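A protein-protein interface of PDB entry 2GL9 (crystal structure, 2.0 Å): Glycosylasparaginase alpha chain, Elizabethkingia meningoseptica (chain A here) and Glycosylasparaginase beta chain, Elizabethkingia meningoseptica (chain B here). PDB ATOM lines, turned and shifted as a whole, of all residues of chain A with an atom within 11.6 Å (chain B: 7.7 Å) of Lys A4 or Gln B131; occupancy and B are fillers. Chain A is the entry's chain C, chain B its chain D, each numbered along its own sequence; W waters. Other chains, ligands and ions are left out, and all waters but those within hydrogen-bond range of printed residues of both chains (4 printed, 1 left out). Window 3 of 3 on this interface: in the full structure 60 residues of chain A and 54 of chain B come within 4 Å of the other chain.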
ATOM      1  N   THR A   2      26.571   1.938  13.376  1.00  0.00           N
ATOM      2  CA  THR A   2      25.346   2.576  13.984  1.00  0.00           C
ATOM      3  C   THR A   2      25.262   4.082  13.721  1.00  0.00           C
ATOM      4  O   THR A   2      26.189   4.826  14.042  1.00  0.00           O
ATOM      5  CB  THR A   2      25.285   2.345  15.524  1.00  0.00           C
ATOM      6  OG1 THR A   2      25.231   0.938  15.793  1.00  0.00           O
ATOM      7  CG2 THR A   2      24.051   3.012  16.134  1.00  0.00           C
ATOM      8  N   ASN A   3      24.146   4.522  13.141  1.00  0.00           N
ATOM      9  CA  ASN A   3      23.910   5.934  12.845  1.00  0.00           C
ATOM     10  C   ASN A   3      23.061   6.490  13.993  1.00  0.00           C
ATOM     11  O   ASN A   3      21.857   6.209  14.078  1.00  0.00           O
ATOM     12  CB  ASN A   3      23.159   6.046  11.516  1.00  0.00           C
ATOM     13  CG  ASN A   3      22.884   7.485  11.100  1.00  0.00           C
ATOM     14  OD1 ASN A   3      23.392   8.442  11.689  1.00  0.00           O
ATOM     15  ND2 ASN A   3      22.066   7.638  10.054  1.00  0.00           N
ATOM     16  N   LYS A   4      23.687   7.250  14.884  1.00  0.00           N
ATOM     17  CA  LYS A   4      22.989   7.808  16.044  1.00  0.00           C
ATOM     18  C   LYS A   4      23.739   9.021  16.576  1.00  0.00           C
ATOM     19  O   LYS A   4      24.957   9.113  16.449  1.00  0.00           O
ATOM     20  CB  LYS A   4      22.851   6.749  17.151  1.00  0.00           C
ATOM     21  CG  LYS A   4      24.158   6.337  17.877  1.00  0.00           C
ATOM     22  CD  LYS A   4      23.868   5.285  18.989  1.00  0.00           C
ATOM     23  CE  LYS A   4      25.126   4.636  19.625  1.00  0.00           C
ATOM     24  NZ  LYS A   4      26.054   5.633  20.198  1.00  0.00           N
ATOM     25  N   PRO A   5      23.023   9.987  17.141  1.00  0.00           N
ATOM     26  CA  PRO A   5      21.561  10.031  17.303  1.00  0.00           C
ATOM     27  C   PRO A   5      20.837  10.254  15.964  1.00  0.00           C
ATOM     28  O   PRO A   5      21.416  10.783  15.011  1.00  0.00           O
ATOM     29  CB  PRO A   5      21.339  11.231  18.235  1.00  0.00           C
ATOM     30  CG  PRO A   5      22.737  11.591  18.761  1.00  0.00           C
ATOM     31  CD  PRO A   5      23.658  11.217  17.641  1.00  0.00           C
ATOM     32  N   ILE A   6      19.583   9.815  15.873  1.00  0.00           N
ATOM     33  CA  ILE A   6      18.790  10.040  14.666  1.00  0.00           C
ATOM     34  C   ILE A   6      17.292  10.139  15.032  1.00  0.00           C
ATOM     35  O   ILE A   6      16.813   9.437  15.947  1.00  0.00           O
ATOM     36  CB  ILE A   6      19.017   8.922  13.593  1.00  0.00           C
ATOM     37  CG1 ILE A   6      18.027   9.108  12.439  1.00  0.00           C
ATOM     38  CG2 ILE A   6      18.879   7.521  14.221  1.00  0.00           C
ATOM     39  CD1 ILE A   6      18.343   8.259  11.181  1.00  0.00           C
ATOM     40  N   VAL A   7      16.570  11.008  14.320  1.00  0.00           N
ATOM     41  CA  VAL A   7      15.135  11.166  14.540  1.00  0.00           C
ATOM     42  C   VAL A   7      14.340  11.254  13.216  1.00  0.00           C
ATOM     43  O   VAL A   7      14.766  11.885  12.220  1.00  0.00           O
ATOM     44  CB  VAL A   7      14.832  12.425  15.398  1.00  0.00           C
ATOM     45  CG1 VAL A   7      15.328  13.661  14.671  1.00  0.00           C
ATOM     46  CG2 VAL A   7      13.282  12.567  15.659  1.00  0.00           C
ATOM     47  N   LEU A   8      13.201  10.570  13.201  1.00  0.00           N
ATOM     48  CA  LEU A   8      12.302  10.585  12.050  1.00  0.00           C
ATOM     49  C   LEU A   8      10.922  11.058  12.490  1.00  0.00           C
ATOM     50  O   LEU A   8      10.470  10.729  13.588  1.00  0.00           O
ATOM     51  CB  LEU A   8      12.159   9.186  11.419  1.00  0.00           C
ATOM     52  CG  LEU A   8      13.165   8.734  10.362  1.00  0.00           C
ATOM     53  CD1 LEU A   8      14.470   8.340  11.041  1.00  0.00           C
ATOM     54  CD2 LEU A   8      12.583   7.524   9.639  1.00  0.00           C
ATOM     55  N   ASN A  18      11.755  18.168  13.694  1.00  0.00           N
ATOM     56  CA  ASN A  18      13.030  17.494  13.943  1.00  0.00           C
ATOM     57  C   ASN A  18      14.079  18.440  14.524  1.00  0.00           C
ATOM     58  O   ASN A  18      14.889  18.041  15.370  1.00  0.00           O
ATOM     59  CB  ASN A  18      13.617  16.876  12.674  1.00  0.00           C
ATOM     60  CG  ASN A  18      12.958  15.567  12.292  1.00  0.00           C
ATOM     61  OD1 ASN A  18      12.037  15.083  12.969  1.00  0.00           O
ATOM     62  ND2 ASN A  18      13.423  14.985  11.184  1.00  0.00           N
ATOM     63  N   ALA A  21      13.655  18.462  18.207  1.00  0.00           N
ATOM     64  CA  ALA A  21      14.079  17.193  18.791  1.00  0.00           C
ATOM     65  C   ALA A  21      15.610  17.118  18.816  1.00  0.00           C
ATOM     66  O   ALA A  21      16.203  16.575  19.750  1.00  0.00           O
ATOM     67  CB  ALA A  21      13.520  16.034  17.969  1.00  0.00           C
ATOM     68  N   TRP A  22      16.235  17.679  17.787  1.00  0.00           N
ATOM     69  CA  TRP A  22      17.690  17.637  17.659  1.00  0.00           C
ATOM     70  C   TRP A  22      18.413  18.459  18.703  1.00  0.00           C
ATOM     71  O   TRP A  22      19.555  18.142  19.042  1.00  0.00           O
ATOM     72  CB  TRP A  22      18.121  18.061  16.248  1.00  0.00           C
ATOM     73  CG  TRP A  22      19.535  17.661  15.892  1.00  0.00           C
ATOM     74  CD1 TRP A  22      20.627  18.489  15.770  1.00  0.00           C
ATOM     75  CD2 TRP A  22      20.012  16.332  15.644  1.00  0.00           C
ATOM     76  NE1 TRP A  22      21.746  17.747  15.463  1.00  0.00           N
ATOM     77  CE2 TRP A  22      21.398  16.424  15.379  1.00  0.00           C
ATOM     78  CE3 TRP A  22      19.397  15.068  15.622  1.00  0.00           C
ATOM     79  CZ2 TRP A  22      22.191  15.298  15.094  1.00  0.00           C
ATOM     80  CZ3 TRP A  22      20.193  13.932  15.336  1.00  0.00           C
ATOM     81  CH2 TRP A  22      21.578  14.071  15.075  1.00  0.00           C
ATOM     82  N   LYS A  23      17.761  19.502  19.213  1.00  0.00           N
ATOM     83  CA  LYS A  23      18.338  20.336  20.267  1.00  0.00           C
ATOM     84  C   LYS A  23      18.582  19.454  21.485  1.00  0.00           C
ATOM     85  O   LYS A  23      19.497  19.702  22.277  1.00  0.00           O
ATOM     86  CB  LYS A  23      17.385  21.466  20.662  1.00  0.00           C
ATOM     87  CG  LYS A  23      17.162  22.511  19.581  1.00  0.00           C
ATOM     88  CD  LYS A  23      16.209  23.584  20.053  1.00  0.00           C
ATOM     89  CE  LYS A  23      16.224  24.761  19.092  1.00  0.00           C
ATOM     90  NZ  LYS A  23      15.163  25.723  19.500  1.00  0.00           N
ATOM     91  N   VAL A  24      17.729  18.442  21.660  1.00  0.00           N
ATOM     92  CA  VAL A  24      17.882  17.503  22.770  1.00  0.00           C
ATOM     93  C   VAL A  24      18.886  16.405  22.351  1.00  0.00           C
ATOM     94  O   VAL A  24      19.885  16.179  23.021  1.00  0.00           O
ATOM     95  CB  VAL A  24      16.508  16.831  23.163  1.00  0.00           C
ATOM     96  CG1 VAL A  24      16.728  15.760  24.208  1.00  0.00           C
ATOM     97  CG2 VAL A  24      15.521  17.896  23.705  1.00  0.00           C
ATOM     98  N   LEU A  25      18.639  15.758  21.216  1.00  0.00           N
ATOM     99  CA  LEU A  25      19.490  14.668  20.767  1.00  0.00           C
ATOM    100  C   LEU A  25      20.964  14.998  20.573  1.00  0.00           C
ATOM    101  O   LEU A  25      21.839  14.194  20.934  1.00  0.00           O
ATOM    102  CB  LEU A  25      18.936  14.083  19.468  1.00  0.00           C
ATOM    103  CG  LEU A  25      17.535  13.446  19.579  1.00  0.00           C
ATOM    104  CD1 LEU A  25      16.992  13.133  18.178  1.00  0.00           C
ATOM    105  CD2 LEU A  25      17.621  12.171  20.452  1.00  0.00           C
ATOM    106  N   SER A  26      21.246  16.159  19.988  1.00  0.00           N
ATOM    107  CA  SER A  26      22.629  16.552  19.736  1.00  0.00           C
ATOM    108  C   SER A  26      23.424  16.840  21.011  1.00  0.00           C
ATOM    109  O   SER A  26      24.624  16.831  20.989  1.00  0.00           O
ATOM    110  CB  SER A  26      22.688  17.777  18.791  1.00  0.00           C
ATOM    111  OG  SER A  26      22.198  18.945  19.437  1.00  0.00           O
ATOM    112  N   LYS A  27      22.757  17.110  22.123  1.00  0.00           N
ATOM    113  CA  LYS A  27      23.480  17.373  23.357  1.00  0.00           C
ATOM    114  C   LYS A  27      23.501  16.126  24.218  1.00  0.00           C
ATOM    115  O   LYS A  27      23.765  16.213  25.414  1.00  0.00           O
ATOM    116  CB  LYS A  27      22.826  18.511  24.142  1.00  0.00           C
ATOM    117  CG  LYS A  27      22.660  19.786  23.350  1.00  0.00           C
ATOM    118  CD  LYS A  27      22.077  20.882  24.231  1.00  0.00           C
ATOM    119  CE  LYS A  27      21.901  22.217  23.470  1.00  0.00           C
ATOM    120  NZ  LYS A  27      20.824  22.167  22.424  1.00  0.00           N
ATOM    121  N   GLY A  28      23.202  14.975  23.618  1.00  0.00           N
ATOM    122  CA  GLY A  28      23.208  13.728  24.371  1.00  0.00           C
ATOM    123  C   GLY A  28      21.971  13.403  25.205  1.00  0.00           C
ATOM    124  O   GLY A  28      21.999  12.441  25.985  1.00  0.00           O
ATOM    125  N   GLY A  29      20.889  14.179  25.044  1.00  0.00           N
ATOM    126  CA  GLY A  29      19.661  13.974  25.798  1.00  0.00           C
ATOM    127  C   GLY A  29      18.899  12.689  25.457  1.00  0.00           C
ATOM    128  O   GLY A  29      19.192  12.014  24.474  1.00  0.00           O
ATOM    129  N   LYS A  30      17.893  12.377  26.257  1.00  0.00           N
ATOM    130  CA  LYS A  30      17.099  11.165  26.074  1.00  0.00           C
ATOM    131  C   LYS A  30      16.147  11.216  24.881  1.00  0.00           C
ATOM    132  O   LYS A  30      15.544  12.261  24.596  1.00  0.00           O
ATOM    133  CB  LYS A  30      16.303  10.913  27.347  1.00  0.00           C
ATOM    134  CG  LYS A  30      17.174  10.479  28.545  1.00  0.00           C
ATOM    135  CD  LYS A  30      16.500  10.782  29.913  1.00  0.00           C
ATOM    136  CE  LYS A  30      15.236  10.002  30.155  1.00  0.00           C
ATOM    137  NZ  LYS A  30      14.478  10.471  31.406  1.00  0.00           N
ATOM    138  N   ALA A  31      16.004  10.080  24.200  1.00  0.00           N
ATOM    139  CA  ALA A  31      15.112   9.990  23.055  1.00  0.00           C
ATOM    140  C   ALA A  31      13.710  10.425  23.500  1.00  0.00           C
ATOM    141  O   ALA A  31      13.015  11.134  22.785  1.00  0.00           O
ATOM    142  CB  ALA A  31      15.072   8.551  22.519  1.00  0.00           C
ATOM    143  N   ALA A  34      13.452  14.140  23.576  1.00  0.00           N
ATOM    144  CA  ALA A  34      13.538  14.665  22.233  1.00  0.00           C
ATOM    145  C   ALA A  34      12.207  14.547  21.479  1.00  0.00           C
ATOM    146  O   ALA A  34      11.752  15.552  20.889  1.00  0.00           O
ATOM    147  CB  ALA A  34      14.627  13.959  21.474  1.00  0.00           C
ATOM    148  N   LEU B   7      16.379   7.579  18.033  1.00  0.00           N
ATOM    149  CA  LEU B   7      17.391   6.699  18.629  1.00  0.00           C
ATOM    150  C   LEU B   7      18.379   7.707  19.187  1.00  0.00           C
ATOM    151  O   LEU B   7      18.916   8.540  18.425  1.00  0.00           O
ATOM    152  CB  LEU B   7      18.079   5.848  17.560  1.00  0.00           C
ATOM    153  CG  LEU B   7      19.260   4.947  18.004  1.00  0.00           C
ATOM    154  CD1 LEU B   7      18.810   3.845  18.984  1.00  0.00           C
ATOM    155  CD2 LEU B   7      19.828   4.293  16.735  1.00  0.00           C
ATOM    156  N   ASP B   8      18.621   7.673  20.492  1.00  0.00           N
ATOM    157  CA  ASP B   8      19.530   8.673  21.078  1.00  0.00           C
ATOM    158  C   ASP B   8      20.982   8.235  21.182  1.00  0.00           C
ATOM    159  O   ASP B   8      21.344   7.151  20.729  1.00  0.00           O
ATOM    160  CB  ASP B   8      19.011   9.185  22.435  1.00  0.00           C
ATOM    161  CG  ASP B   8      18.915   8.089  23.515  1.00  0.00           C
ATOM    162  OD1 ASP B   8      19.730   7.129  23.515  1.00  0.00           O
ATOM    163  OD2 ASP B   8      18.021   8.213  24.386  1.00  0.00           O
ATOM    164  N   ALA B   9      21.807   9.097  21.760  1.00  0.00           N
ATOM    165  CA  ALA B   9      23.236   8.828  21.893  1.00  0.00           C
ATOM    166  C   ALA B   9      23.527   7.574  22.721  1.00  0.00           C
ATOM    167  O   ALA B   9      24.567   6.953  22.527  1.00  0.00           O
ATOM    168  CB  ALA B   9      23.956  10.061  22.512  1.00  0.00           C
ATOM    169  N   GLN B  10      22.620   7.215  23.640  1.00  0.00           N
ATOM    170  CA  GLN B  10      22.804   6.011  24.453  1.00  0.00           C
ATOM    171  C   GLN B  10      22.403   4.774  23.662  1.00  0.00           C
ATOM    172  O   GLN B  10      22.607   3.637  24.104  1.00  0.00           O
ATOM    173  CB  GLN B  10      21.962   6.074  25.727  1.00  0.00           C
ATOM    174  CG  GLN B  10      22.390   7.183  26.672  1.00  0.00           C
ATOM    175  CD  GLN B  10      21.356   7.441  27.744  1.00  0.00           C
ATOM    176  OE1 GLN B  10      21.214   6.662  28.697  1.00  0.00           O
ATOM    177  NE2 GLN B  10      20.607   8.525  27.583  1.00  0.00           N
ATOM    178  N   GLY B  11      21.825   4.996  22.493  1.00  0.00           N
ATOM    179  CA  GLY B  11      21.404   3.868  21.682  1.00  0.00           C
ATOM    180  C   GLY B  11      19.998   3.436  22.057  1.00  0.00           C
ATOM    181  O   GLY B  11      19.598   2.302  21.779  1.00  0.00           O
ATOM    182  N   ASN B  12      19.259   4.331  22.708  1.00  0.00           N
ATOM    183  CA  ASN B  12      17.879   4.045  23.128  1.00  0.00           C
ATOM    184  C   ASN B  12      16.822   4.653  22.198  1.00  0.00           C
ATOM    185  O   ASN B  12      16.965   5.778  21.708  1.00  0.00           O
ATOM    186  CB  ASN B  12      17.590   4.591  24.526  1.00  0.00           C
ATOM    187  CG  ASN B  12      18.260   3.782  25.606  1.00  0.00           C
ATOM    188  OD1 ASN B  12      18.492   2.584  25.437  1.00  0.00           O
ATOM    189  ND2 ASN B  12      18.561   4.431  26.729  1.00  0.00           N
ATOM    190  N   LYS B 111      17.582  -0.596  15.750  1.00  0.00           N
ATOM    191  CA  LYS B 111      18.613  -0.291  16.737  1.00  0.00           C
ATOM    192  C   LYS B 111      19.918   0.177  16.155  1.00  0.00           C
ATOM    193  O   LYS B 111      20.711   0.785  16.861  1.00  0.00           O
ATOM    194  CB  LYS B 111      18.880  -1.492  17.654  1.00  0.00           C
ATOM    195  CG  LYS B 111      17.866  -1.606  18.764  1.00  0.00           C
ATOM    196  CD  LYS B 111      18.014  -0.501  19.841  1.00  0.00           C
ATOM    197  CE  LYS B 111      19.011  -0.912  20.906  1.00  0.00           C
ATOM    198  NZ  LYS B 111      18.660  -0.301  22.209  1.00  0.00           N
ATOM    199  N   LYS B 112      20.162  -0.122  14.890  1.00  0.00           N
ATOM    200  CA  LYS B 112      21.400   0.321  14.261  1.00  0.00           C
ATOM    201  C   LYS B 112      21.252   1.737  13.694  1.00  0.00           C
ATOM    202  O   LYS B 112      22.175   2.294  13.108  1.00  0.00           O
ATOM    203  CB  LYS B 112      21.793  -0.640  13.137  1.00  0.00           C
ATOM    204  CG  LYS B 112      22.054  -2.065  13.586  1.00  0.00           C
ATOM    205  CD  LYS B 112      22.483  -2.953  12.387  1.00  0.00           C
ATOM    206  CE  LYS B 112      21.310  -3.287  11.394  1.00  0.00           C
ATOM    207  NZ  LYS B 112      20.302  -4.319  11.894  1.00  0.00           N
ATOM    208  N   GLY B 113      20.095   2.352  13.865  1.00  0.00           N
ATOM    209  CA  GLY B 113      19.989   3.681  13.300  1.00  0.00           C
ATOM    210  C   GLY B 113      19.604   3.669  11.830  1.00  0.00           C
ATOM    211  O   GLY B 113      19.467   4.751  11.234  1.00  0.00           O
ATOM    212  N   GLU B 114      19.440   2.487  11.230  1.00  0.00           N
ATOM    213  CA  GLU B 114      18.988   2.382   9.827  1.00  0.00           C
ATOM    214  C   GLU B 114      17.476   2.727   9.868  1.00  0.00           C
ATOM    215  O   GLU B 114      16.807   2.414  10.843  1.00  0.00           O
ATOM    216  CB  GLU B 114      19.157   0.970   9.306  1.00  0.00           C
ATOM    217  CG  GLU B 114      20.620   0.543   9.178  1.00  0.00           C
ATOM    218  CD  GLU B 114      20.779  -0.963   9.055  1.00  0.00           C
ATOM    219  OE1 GLU B 114      21.924  -1.414   8.829  1.00  0.00           O
ATOM    220  OE2 GLU B 114      19.779  -1.704   9.196  1.00  0.00           O
ATOM    221  N   HIS B 129      16.590  13.427  10.495  1.00  0.00           N
ATOM    222  CA  HIS B 129      17.716  14.258  10.931  1.00  0.00           C
ATOM    223  C   HIS B 129      18.684  13.329  11.651  1.00  0.00           C
ATOM    224  O   HIS B 129      18.298  12.626  12.585  1.00  0.00           O
ATOM    225  CB  HIS B 129      17.216  15.314  11.929  1.00  0.00           C
ATOM    226  CG  HIS B 129      18.156  16.464  12.149  1.00  0.00           C
ATOM    227  ND1 HIS B 129      19.529  16.337  12.117  1.00  0.00           N
ATOM    228  CD2 HIS B 129      17.902  17.765  12.421  1.00  0.00           C
ATOM    229  CE1 HIS B 129      20.080  17.515  12.349  1.00  0.00           C
ATOM    230  NE2 HIS B 129      19.117  18.400  12.538  1.00  0.00           N
ATOM    231  N   ASP B 130      19.921  13.293  11.188  1.00  0.00           N
ATOM    232  CA  ASP B 130      20.964  12.510  11.828  1.00  0.00           C
ATOM    233  C   ASP B 130      22.199  13.440  11.815  1.00  0.00           C
ATOM    234  O   ASP B 130      22.045  14.644  11.606  1.00  0.00           O
ATOM    235  CB  ASP B 130      21.215  11.202  11.073  1.00  0.00           C
ATOM    236  CG  ASP B 130      21.587  11.424   9.627  1.00  0.00           C
ATOM    237  OD1 ASP B 130      21.588  10.437   8.866  1.00  0.00           O
ATOM    238  OD2 ASP B 130      21.880  12.583   9.249  1.00  0.00           O
ATOM    239  N   GLN B 131      23.399  12.922  12.051  1.00  0.00           N
ATOM    240  CA  GLN B 131      24.571  13.802  12.062  1.00  0.00           C
ATOM    241  C   GLN B 131      24.874  14.466  10.722  1.00  0.00           C
ATOM    242  O   GLN B 131      25.504  15.520  10.685  1.00  0.00           O
ATOM    243  CB  GLN B 131      25.801  13.057  12.592  1.00  0.00           C
ATOM    244  CG  GLN B 131      25.722  12.901  14.110  1.00  0.00           C
ATOM    245  CD  GLN B 131      26.908  12.175  14.730  1.00  0.00           C
ATOM    246  OE1 GLN B 131      28.062  12.476  14.429  1.00  0.00           O
ATOM    247  NE2 GLN B 131      26.627  11.227  15.619  1.00  0.00           N
ATOM    248  N   LYS B 132      24.404  13.876   9.628  1.00  0.00           N
ATOM    249  CA  LYS B 132      24.645  14.482   8.333  1.00  0.00           C
ATOM    250  C   LYS B 132      23.712  15.665   8.073  1.00  0.00           C
ATOM    251  O   LYS B 132      23.928  16.417   7.124  1.00  0.00           O
ATOM    252  CB  LYS B 132      24.495  13.437   7.235  1.00  0.00           C
ATOM    253  CG  LYS B 132      25.460  12.267   7.413  1.00  0.00           C
ATOM    254  CD  LYS B 132      26.900  12.766   7.560  1.00  0.00           C
ATOM    255  CE  LYS B 132      27.905  11.616   7.809  1.00  0.00           C
ATOM    256  NZ  LYS B 132      27.865  10.568   6.735  1.00  0.00           N
ATOM    257  N   GLY B 133      22.687  15.842   8.912  1.00  0.00           N
ATOM    258  CA  GLY B 133      21.762  16.952   8.722  1.00  0.00           C
ATOM    259  C   GLY B 133      20.284  16.557   8.688  1.00  0.00           C
ATOM    260  O   GLY B 133      19.930  15.406   8.909  1.00  0.00           O
ATOM    261  N   ASN B 134      19.425  17.517   8.395  1.00  0.00           N
ATOM    262  CA  ASN B 134      17.980  17.280   8.385  1.00  0.00           C
ATOM    263  C   ASN B 134      17.460  17.267   6.961  1.00  0.00           C
ATOM    264  O   ASN B 134      17.736  18.200   6.202  1.00  0.00           O
ATOM    265  CB  ASN B 134      17.315  18.405   9.184  1.00  0.00           C
ATOM    266  CG  ASN B 134      15.895  18.076   9.624  1.00  0.00           C
ATOM    267  OD1 ASN B 134      15.535  16.914   9.784  1.00  0.00           O
ATOM    268  ND2 ASN B 134      15.087  19.123   9.842  1.00  0.00           N
ATOM    269  N   ARG B 135      16.730  16.220   6.579  1.00  0.00           N
ATOM    270  CA  ARG B 135      16.181  16.182   5.232  1.00  0.00           C
ATOM    271  C   ARG B 135      14.807  15.590   5.042  1.00  0.00           C
ATOM    272  O   ARG B 135      14.337  14.781   5.833  1.00  0.00           O
ATOM    273  CB  ARG B 135      17.154  15.510   4.270  1.00  0.00           C
ATOM    274  CG  ARG B 135      17.382  14.102   4.511  1.00  0.00           C
ATOM    275  CD  ARG B 135      18.873  13.800   4.672  1.00  0.00           C
ATOM    276  NE  ARG B 135      19.034  12.412   5.154  1.00  0.00           N
ATOM    277  CZ  ARG B 135      19.820  12.054   6.163  1.00  0.00           C
ATOM    278  NH1 ARG B 135      20.560  12.955   6.812  1.00  0.00           N
ATOM    279  NH2 ARG B 135      19.804  10.800   6.597  1.00  0.00           N
HETATM  280  O   HOH W   1      21.023   5.465   8.808  1.00  0.00           O
HETATM  281  O   HOH W   2      21.083  11.865  22.429  1.00  0.00           O
HETATM  282  O   HOH W   3      25.007  10.338  10.348  1.00  0.00           O
HETATM  283  O   HOH W   4      23.716  10.407  13.472  1.00  0.00           O
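The backbone carbonyl oxygen of Lys B112 is in hydrogen-bond range of the backbone NH of Asn A3 (3.0 Å). ND2 of Asn A3 lies within hydrogen-bond range of OD1 of Asp B130, at 3.1 Å. The side-chain amino group of Lys A4 sits at hydrogen-bond distance from the backbone carbonyl oxygen of Ala B9, 3.1 Å away. The backbone carbonyl oxygen (O) of Lys A4 sits at hydrogen-bond distance from the side-chain amide nitrogen (NE2) of Gln B131 (2.8 Å). The backbone carbonyl oxygen (O) of Ile A6 sits at hydrogen-bond distance from the backbone NH (N) of Leu B7, at 2.8 Å. N of Val A7 is in hydrogen-bond range of O of His B129 (2.9 Å). OD1 of Asn B134 sits at hydrogen-bond distance from ND2 of Asn A18 (3.2 Å). The side-chain carboxylate (OD2) of Asp B8 sits at hydrogen-bond distance from the backbone NH (N) of Ala A31, 2.8 Å away.
O of Val A24 is in hydrogen-bond range of N of Gly A29 (3.0 Å). The side-chain carboxylate of Asp B8 lies within hydrogen-bond range of the backbone NH of Gln B10 (2.9 Å). The side-chain carboxylate (OD1) of Asp B8 lies within hydrogen-bond range of the backbone NH (N) of Gly B11, 3.2 Å away. The backbone carbonyl oxygen (O) of Gly B11 is in hydrogen-bond range of the side-chain amino group (NZ) of Lys B111 (2.8 Å). OE2 of Glu B114 lies within salt-bridge range of NZ of Lys B112. OD2 of Asp B130 is in hydrogen-bond range of N of Gly B133, at 3.4 Å.
Lys B112 touches Thr A2. Asn A3 touches Gly B113. Lys A4 touches Asp B8. Leu B7 touches Pro A5 (O to CA, 3.2 Å). Ile A6 touches Gly B113 (CD1 to O, 3.7 Å). His B129 touches Trp A22. Trp A22 touches Asp B130 (CH2 to C, 3.4 Å). CB of Asp B8 touches CD2 of Leu A25, 3.8 Å away. Gly A29 touches Asp B8. CA of Lys A30 touches OD2 of Asp B8, at 3.5 Å.
Lys A4 touches just these residues of chain B: Leu B7, Asp B8, Ala B9, Gly B11 and Gln B131. Gln B131 touches just these residues of chain A: Lys A4, Pro A5 and Trp A22. Leu B7 touches four residues of chain A. Gly B11 touches just one residue of chain A: Lys A4. His B129 touches four residues of chain A. Asp B130 touches three residues of chain A. No residue of chain A comes within 4 Å of Lys B132. Of the printed residues of chain A, Asn B134 touches Asn A18 (3.2 Å). Printed residues of chain A within 4 Å of Ala B9: Lys A4. Of the printed residues of chain A, Lys B112 touches Thr A2 (3.3 Å) and Asn A3 (3.0 Å). Ala A21 touches none of the printed residues of chain B. Gly A28 touches none of the printed residues of chain B.
Of the 17 printed residues of chain B, 11 touch a printed residue of chain A. Among the printed residues, 27 pairs touch across the chains. Among the printed residues, no Asp or Glu carboxylate lies within 4 Å of a Lys or Arg side-chain nitrogen of the other chain.
Water W4 lies within hydrogen-bond range of OD1 of Asn A3 (2.7 Å), O of Pro A5 (2.8 Å), N of Gln B131 (2.9 Å) and N of Lys A4 (3.5 Å). Water W1 bridges the side-chain amide nitrogen (ND2) of Asn A3 (2.7 Å) and the backbone carbonyl oxygen (O) of Gly B113 (3.0 Å). Water W2 lies within hydrogen-bond range of O of Gly A29 (2.8 Å), O of Leu A25 (2.9 Å) and N of Ala B9 (2.9 Å). Water W3 bridges the side-chain amide oxygen (OD1) of Asn A3 (2.8 Å) and the backbone NH (N) of Gln B131 (3.5 Å).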
